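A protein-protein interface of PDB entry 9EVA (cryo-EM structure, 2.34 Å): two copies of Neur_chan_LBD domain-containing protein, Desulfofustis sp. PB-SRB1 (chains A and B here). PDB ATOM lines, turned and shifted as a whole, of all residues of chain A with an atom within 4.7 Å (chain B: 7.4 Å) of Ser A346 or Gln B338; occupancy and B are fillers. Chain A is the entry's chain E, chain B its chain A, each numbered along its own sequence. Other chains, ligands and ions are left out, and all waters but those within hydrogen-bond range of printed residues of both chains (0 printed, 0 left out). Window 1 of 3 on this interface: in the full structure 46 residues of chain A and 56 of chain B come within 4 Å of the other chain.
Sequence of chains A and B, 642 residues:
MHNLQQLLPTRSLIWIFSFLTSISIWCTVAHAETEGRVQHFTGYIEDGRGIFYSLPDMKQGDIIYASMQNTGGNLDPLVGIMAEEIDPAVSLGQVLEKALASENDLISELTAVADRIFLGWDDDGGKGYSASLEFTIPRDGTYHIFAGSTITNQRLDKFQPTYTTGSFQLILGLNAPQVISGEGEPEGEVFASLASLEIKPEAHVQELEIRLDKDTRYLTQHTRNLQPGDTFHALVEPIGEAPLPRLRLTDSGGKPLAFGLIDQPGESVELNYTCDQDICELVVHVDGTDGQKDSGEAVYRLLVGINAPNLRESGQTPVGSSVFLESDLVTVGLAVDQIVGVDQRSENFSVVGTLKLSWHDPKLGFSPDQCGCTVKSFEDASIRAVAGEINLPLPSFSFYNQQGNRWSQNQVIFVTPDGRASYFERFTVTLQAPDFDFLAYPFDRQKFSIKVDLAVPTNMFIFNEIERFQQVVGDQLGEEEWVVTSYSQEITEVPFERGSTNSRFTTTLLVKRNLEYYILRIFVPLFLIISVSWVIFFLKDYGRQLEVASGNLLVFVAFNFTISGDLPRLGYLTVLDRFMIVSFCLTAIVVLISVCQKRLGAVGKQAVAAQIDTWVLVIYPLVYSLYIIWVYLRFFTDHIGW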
ATOM      1  N   ASP A 343      -6.715 -17.166 -25.343  1.00  0.00           N
ATOM      2  CA  ASP A 343      -6.864 -17.860 -26.619  1.00  0.00           C
ATOM      3  C   ASP A 343      -7.664 -16.961 -27.553  1.00  0.00           C
ATOM      4  O   ASP A 343      -8.869 -16.772 -27.359  1.00  0.00           O
ATOM      5  CB  ASP A 343      -7.548 -19.212 -26.423  1.00  0.00           C
ATOM      6  CG  ASP A 343      -7.390 -20.131 -27.618  1.00  0.00           C
ATOM      7  OD1 ASP A 343      -7.187 -19.632 -28.745  1.00  0.00           O
ATOM      8  OD2 ASP A 343      -7.471 -21.362 -27.431  1.00  0.00           O
ATOM      9  N   GLN A 344      -6.998 -16.414 -28.572  1.00  0.00           N
ATOM     10  CA  GLN A 344      -7.626 -15.415 -29.426  1.00  0.00           C
ATOM     11  C   GLN A 344      -8.489 -16.017 -30.528  1.00  0.00           C
ATOM     12  O   GLN A 344      -9.314 -15.302 -31.106  1.00  0.00           O
ATOM     13  CB  GLN A 344      -6.556 -14.513 -30.043  1.00  0.00           C
ATOM     14  CG  GLN A 344      -5.696 -13.802 -29.015  1.00  0.00           C
ATOM     15  CD  GLN A 344      -4.599 -12.967 -29.638  1.00  0.00           C
ATOM     16  OE1 GLN A 344      -4.040 -12.080 -28.998  1.00  0.00           O
ATOM     17  NE2 GLN A 344      -4.281 -13.251 -30.896  1.00  0.00           N
ATOM     18  N   ARG A 345      -8.330 -17.304 -30.832  1.00  0.00           N
ATOM     19  CA  ARG A 345      -9.179 -17.938 -31.834  1.00  0.00           C
ATOM     20  C   ARG A 345     -10.459 -18.508 -31.235  1.00  0.00           C
ATOM     21  O   ARG A 345     -11.533 -18.363 -31.827  1.00  0.00           O
ATOM     22  CB  ARG A 345      -8.411 -19.040 -32.565  1.00  0.00           C
ATOM     23  CG  ARG A 345      -7.511 -18.534 -33.676  1.00  0.00           C
ATOM     24  CD  ARG A 345      -6.883 -19.682 -34.449  1.00  0.00           C
ATOM     25  NE  ARG A 345      -7.885 -20.570 -35.025  1.00  0.00           N
ATOM     26  CZ  ARG A 345      -8.425 -20.414 -36.226  1.00  0.00           C
ATOM     27  NH1 ARG A 345      -8.087 -19.405 -37.010  1.00  0.00           N
ATOM     28  NH2 ARG A 345      -9.329 -21.293 -36.650  1.00  0.00           N
ATOM     29  N   SER A 346     -10.370 -19.152 -30.075  1.00  0.00           N
ATOM     30  CA  SER A 346     -11.540 -19.692 -29.397  1.00  0.00           C
ATOM     31  C   SER A 346     -12.167 -18.703 -28.423  1.00  0.00           C
ATOM     32  O   SER A 346     -13.250 -18.979 -27.899  1.00  0.00           O
ATOM     33  CB  SER A 346     -11.170 -20.983 -28.660  1.00  0.00           C
ATOM     34  OG  SER A 346     -12.290 -21.525 -27.984  1.00  0.00           O
ATOM     35  N   GLU A 347     -11.515 -17.566 -28.180  1.00  0.00           N
ATOM     36  CA  GLU A 347     -12.045 -16.481 -27.354  1.00  0.00           C
ATOM     37  C   GLU A 347     -12.363 -16.952 -25.932  1.00  0.00           C
ATOM     38  O   GLU A 347     -13.510 -16.942 -25.480  1.00  0.00           O
ATOM     39  CB  GLU A 347     -13.266 -15.840 -28.022  1.00  0.00           C
ATOM     40  CG  GLU A 347     -12.963 -15.269 -29.397  1.00  0.00           C
ATOM     41  CD  GLU A 347     -14.113 -14.474 -29.975  1.00  0.00           C
ATOM     42  OE1 GLU A 347     -15.034 -14.117 -29.213  1.00  0.00           O
ATOM     43  OE2 GLU A 347     -14.097 -14.205 -31.194  1.00  0.00           O
ATOM     44  N   ASN A 348     -11.312 -17.364 -25.226  1.00  0.00           N
ATOM     45  CA  ASN A 348     -11.404 -17.711 -23.816  1.00  0.00           C
ATOM     46  C   ASN A 348     -10.099 -17.337 -23.126  1.00  0.00           C
ATOM     47  O   ASN A 348      -9.059 -17.165 -23.768  1.00  0.00           O
ATOM     48  CB  ASN A 348     -11.724 -19.200 -23.616  1.00  0.00           C
ATOM     49  CG  ASN A 348     -10.658 -20.112 -24.188  1.00  0.00           C
ATOM     50  OD1 ASN A 348      -9.618 -20.329 -23.573  1.00  0.00           O
ATOM     51  ND2 ASN A 348     -10.921 -20.663 -25.362  1.00  0.00           N
ATOM     52  N   PRO A 434     -16.975 -14.551 -25.493  1.00  0.00           N
ATOM     53  CA  PRO A 434     -17.307 -14.138 -26.867  1.00  0.00           C
ATOM     54  C   PRO A 434     -17.358 -12.632 -27.064  1.00  0.00           C
ATOM     55  O   PRO A 434     -17.552 -12.179 -28.198  1.00  0.00           O
ATOM     56  CB  PRO A 434     -18.678 -14.783 -27.103  1.00  0.00           C
ATOM     57  CG  PRO A 434     -19.255 -14.939 -25.745  1.00  0.00           C
ATOM     58  CD  PRO A 434     -18.105 -15.222 -24.829  1.00  0.00           C
ATOM     59  N   ALA B 335     -30.990 -23.519 -29.036  1.00  0.00           N
ATOM     60  CA  ALA B 335     -30.387 -22.246 -29.405  1.00  0.00           C
ATOM     61  C   ALA B 335     -28.872 -22.390 -29.459  1.00  0.00           C
ATOM     62  O   ALA B 335     -28.281 -23.109 -28.649  1.00  0.00           O
ATOM     63  CB  ALA B 335     -30.774 -21.140 -28.417  1.00  0.00           C
ATOM     64  N   VAL B 336     -28.249 -21.707 -30.417  1.00  0.00           N
ATOM     65  CA  VAL B 336     -26.802 -21.738 -30.609  1.00  0.00           C
ATOM     66  C   VAL B 336     -26.221 -20.406 -30.156  1.00  0.00           C
ATOM     67  O   VAL B 336     -26.678 -19.341 -30.590  1.00  0.00           O
ATOM     68  CB  VAL B 336     -26.439 -22.024 -32.076  1.00  0.00           C
ATOM     69  CG1 VAL B 336     -24.960 -21.778 -32.314  1.00  0.00           C
ATOM     70  CG2 VAL B 336     -26.808 -23.450 -32.451  1.00  0.00           C
ATOM     71  N   ASP B 337     -25.214 -20.461 -29.286  1.00  0.00           N
ATOM     72  CA  ASP B 337     -24.577 -19.254 -28.770  1.00  0.00           C
ATOM     73  C   ASP B 337     -23.302 -18.897 -29.528  1.00  0.00           C
ATOM     74  O   ASP B 337     -23.119 -17.742 -29.925  1.00  0.00           O
ATOM     75  CB  ASP B 337     -24.275 -19.416 -27.277  1.00  0.00           C
ATOM     76  CG  ASP B 337     -25.532 -19.562 -26.442  1.00  0.00           C
ATOM     77  OD1 ASP B 337     -26.573 -18.988 -26.827  1.00  0.00           O
ATOM     78  OD2 ASP B 337     -25.480 -20.252 -25.402  1.00  0.00           O
ATOM     79  N   GLN B 338     -22.416 -19.867 -29.745  1.00  0.00           N
ATOM     80  CA  GLN B 338     -21.123 -19.580 -30.354  1.00  0.00           C
ATOM     81  C   GLN B 338     -20.561 -20.838 -30.997  1.00  0.00           C
ATOM     82  O   GLN B 338     -20.608 -21.916 -30.397  1.00  0.00           O
ATOM     83  CB  GLN B 338     -20.143 -19.038 -29.307  1.00  0.00           C
ATOM     84  CG  GLN B 338     -18.732 -18.829 -29.820  1.00  0.00           C
ATOM     85  CD  GLN B 338     -17.761 -18.459 -28.719  1.00  0.00           C
ATOM     86  OE1 GLN B 338     -18.126 -18.406 -27.545  1.00  0.00           O
ATOM     87  NE2 GLN B 338     -16.514 -18.199 -29.094  1.00  0.00           N
ATOM     88  N   ILE B 339     -20.039 -20.697 -32.214  1.00  0.00           N
ATOM     89  CA  ILE B 339     -19.236 -21.740 -32.845  1.00  0.00           C
ATOM     90  C   ILE B 339     -17.790 -21.526 -32.413  1.00  0.00           C
ATOM     91  O   ILE B 339     -17.195 -20.484 -32.700  1.00  0.00           O
ATOM     92  CB  ILE B 339     -19.371 -21.709 -34.372  1.00  0.00           C
ATOM     93  CG1 ILE B 339     -20.823 -21.956 -34.781  1.00  0.00           C
ATOM     94  CG2 ILE B 339     -18.453 -22.735 -35.010  1.00  0.00           C
ATOM     95  CD1 ILE B 339     -21.076 -21.775 -36.254  1.00  0.00           C
ATOM     96  N   VAL B 340     -17.214 -22.514 -31.721  1.00  0.00           N
ATOM     97  CA  VAL B 340     -15.923 -22.327 -31.063  1.00  0.00           C
ATOM     98  C   VAL B 340     -14.767 -23.013 -31.778  1.00  0.00           C
ATOM     99  O   VAL B 340     -13.617 -22.878 -31.327  1.00  0.00           O
ATOM    100  CB  VAL B 340     -15.971 -22.798 -29.593  1.00  0.00           C
ATOM    101  CG1 VAL B 340     -16.913 -21.922 -28.788  1.00  0.00           C
ATOM    102  CG2 VAL B 340     -16.398 -24.247 -29.511  1.00  0.00           C
ATOM    103  N   GLY B 341     -15.015 -23.736 -32.859  1.00  0.00           N
ATOM    104  CA  GLY B 341     -13.919 -24.343 -33.591  1.00  0.00           C
ATOM    105  C   GLY B 341     -14.418 -25.203 -34.732  1.00  0.00           C
ATOM    106  O   GLY B 341     -15.517 -25.766 -34.684  1.00  0.00           O
ATOM    107  N   SER B 350     -17.206 -27.718 -33.173  1.00  0.00           N
ATOM    108  CA  SER B 350     -17.654 -27.608 -31.791  1.00  0.00           C
ATOM    109  C   SER B 350     -18.537 -26.377 -31.622  1.00  0.00           C
ATOM    110  O   SER B 350     -18.291 -25.336 -32.239  1.00  0.00           O
ATOM    111  CB  SER B 350     -16.463 -27.539 -30.834  1.00  0.00           C
ATOM    112  OG  SER B 350     -15.674 -28.712 -30.917  1.00  0.00           O
ATOM    113  N   VAL B 351     -19.567 -26.501 -30.783  1.00  0.00           N
ATOM    114  CA  VAL B 351     -20.595 -25.476 -30.644  1.00  0.00           C
ATOM    115  C   VAL B 351     -21.057 -25.399 -29.191  1.00  0.00           C
ATOM    116  O   VAL B 351     -21.030 -26.390 -28.456  1.00  0.00           O
ATOM    117  CB  VAL B 351     -21.784 -25.753 -31.599  1.00  0.00           C
ATOM    118  CG1 VAL B 351     -22.493 -27.042 -31.220  1.00  0.00           C
ATOM    119  CG2 VAL B 351     -22.751 -24.581 -31.630  1.00  0.00           C
ATOM    120  N   VAL B 352     -21.465 -24.199 -28.776  1.00  0.00           N
ATOM    121  CA  VAL B 352     -21.999 -23.936 -27.442  1.00  0.00           C
ATOM    122  C   VAL B 352     -23.450 -23.487 -27.587  1.00  0.00           C
ATOM    123  O   VAL B 352     -23.755 -22.630 -28.423  1.00  0.00           O
ATOM    124  CB  VAL B 352     -21.168 -22.870 -26.704  1.00  0.00           C
ATOM    125  CG1 VAL B 352     -21.724 -22.624 -25.315  1.00  0.00           C
ATOM    126  CG2 VAL B 352     -19.711 -23.286 -26.630  1.00  0.00           C
ATOM    127  N   GLY B 353     -24.338 -24.057 -26.779  1.00  0.00           N
ATOM    128  CA  GLY B 353     -25.741 -23.715 -26.900  1.00  0.00           C
ATOM    129  C   GLY B 353     -26.562 -24.179 -25.716  1.00  0.00           C
ATOM    130  O   GLY B 353     -26.029 -24.597 -24.687  1.00  0.00           O
ATOM    131  N   PHE B 427     -24.802 -26.753 -22.879  1.00  0.00           N
ATOM    132  CA  PHE B 427     -23.876 -27.767 -23.362  1.00  0.00           C
ATOM    133  C   PHE B 427     -22.756 -27.162 -24.199  1.00  0.00           C
ATOM    134  O   PHE B 427     -22.925 -26.124 -24.845  1.00  0.00           O
ATOM    135  CB  PHE B 427     -24.612 -28.831 -24.195  1.00  0.00           C
ATOM    136  CG  PHE B 427     -25.297 -28.285 -25.420  1.00  0.00           C
ATOM    137  CD1 PHE B 427     -24.621 -28.182 -26.624  1.00  0.00           C
ATOM    138  CD2 PHE B 427     -26.620 -27.886 -25.368  1.00  0.00           C
ATOM    139  CE1 PHE B 427     -25.249 -27.682 -27.747  1.00  0.00           C
ATOM    140  CE2 PHE B 427     -27.251 -27.389 -26.490  1.00  0.00           C
ATOM    141  CZ  PHE B 427     -26.565 -27.286 -27.679  1.00  0.00           C
ATOM    142  N   THR B 428     -21.606 -27.832 -24.169  1.00  0.00           N
ATOM    143  CA  THR B 428     -20.518 -27.618 -25.117  1.00  0.00           C
ATOM    144  C   THR B 428     -20.119 -28.979 -25.667  1.00  0.00           C
ATOM    145  O   THR B 428     -19.745 -29.871 -24.898  1.00  0.00           O
ATOM    146  CB  THR B 428     -19.321 -26.928 -24.454  1.00  0.00           C
ATOM    147  OG1 THR B 428     -19.716 -25.638 -23.971  1.00  0.00           O
ATOM    148  CG2 THR B 428     -18.181 -26.764 -25.444  1.00  0.00           C
ATOM    149  N   GLY B 474     -27.361 -16.639 -32.048  1.00  0.00           N
ATOM    150  CA  GLY B 474     -27.134 -15.458 -31.230  1.00  0.00           C
ATOM    151  C   GLY B 474     -26.062 -14.546 -31.808  1.00  0.00           C
ATOM    152  O   GLY B 474     -25.077 -14.994 -32.394  1.00  0.00           O
ATOM    153  N   GLN B 476     -23.009 -11.804 -31.464  1.00  0.00           N
ATOM    154  CA  GLN B 476     -21.884 -11.560 -30.574  1.00  0.00           C
ATOM    155  C   GLN B 476     -21.081 -10.376 -31.089  1.00  0.00           C
ATOM    156  O   GLN B 476     -21.067 -10.103 -32.292  1.00  0.00           O
ATOM    157  CB  GLN B 476     -20.974 -12.791 -30.457  1.00  0.00           C
ATOM    158  CG  GLN B 476     -21.670 -14.052 -29.968  1.00  0.00           C
ATOM    159  CD  GLN B 476     -22.049 -13.988 -28.501  1.00  0.00           C
ATOM    160  OE1 GLN B 476     -21.617 -13.098 -27.772  1.00  0.00           O
ATOM    161  NE2 GLN B 476     -22.863 -14.940 -28.062  1.00  0.00           N
ATOM    162  N   GLU B 480     -16.506 -12.808 -36.803  1.00  0.00           N
ATOM    163  CA  GLU B 480     -16.337 -14.249 -36.705  1.00  0.00           C
ATOM    164  C   GLU B 480     -15.780 -14.790 -38.014  1.00  0.00           C
ATOM    165  O   GLU B 480     -15.933 -14.176 -39.073  1.00  0.00           O
ATOM    166  CB  GLU B 480     -17.661 -14.953 -36.372  1.00  0.00           C
ATOM    167  CG  GLU B 480     -18.174 -14.706 -34.959  1.00  0.00           C
ATOM    168  CD  GLU B 480     -18.906 -13.387 -34.817  1.00  0.00           C
ATOM    169  OE1 GLU B 480     -19.338 -12.830 -35.847  1.00  0.00           O
ATOM    170  OE2 GLU B 480     -19.050 -12.906 -33.674  1.00  0.00           O
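Of chain B, only Gln B338 (3.6 Å) and Val B340 (3.8 Å) come within 4 Å of Ser A346. Of the printed residues of chain B, Pro A434 touches Gln B338 (3.7 Å) and Gln B476 (3.5 Å). Gln B338 touches just these residues of chain A: Ser A346 (3.6 Å) and Pro A434 (3.7 Å). Of the printed residues of chain A, Val B340 touches Ser A346 (3.8 Å). Of the printed residues of chain A, Gln B476 touches Pro A434 (3.5 Å). The nearest residue of chain B that does not touch Ser A346 is Gly B341 (6.0 Å). The nearest printed residue of chain A that does not touch Gln B476 is Glu A347 (6.2 Å).
Hydrophobic or aromatic side chains of chain A within 4 Å of the printed part of chain B: Pro A434. Among the printed residues, 4 pairs touch across the chains.
Ser A346 touches Gln B338 (O to NE2, 3.6 Å). OG of Ser A346 touches O of Val B340 (3.8 Å). OE1 of Gln B338 touches CB of Pro A434, 3.7 Å away. Pro A434 touches Gln B476 (CB to OE1, 3.5 Å).
No position is printed for both chains. Of the 4 pairs that touch across the chains among the printed residues, none has its exchanged pair printed and touching as well.
The backbone carbonyl oxygen (O) of Ser B350 sits at hydrogen-bond distance from the backbone NH (N) of Val B340 (3.1 Å). OD1 of Asp A343 sits at hydrogen-bond distance from N of Ser A346 (3.5 Å). O of Gln B338 sits at hydrogen-bond distance from N of Val B352 (2.9 Å). The side-chain hydroxyl (OG) of Ser A346 lies within hydrogen-bond range of the side-chain amide nitrogen (ND2) of Asn A348, at 3.1 Å. The side-chain amide nitrogen (NE2) of Gln B476 is in hydrogen-bond range of the backbone carbonyl oxygen (O) of Asp B337 (3.4 Å).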
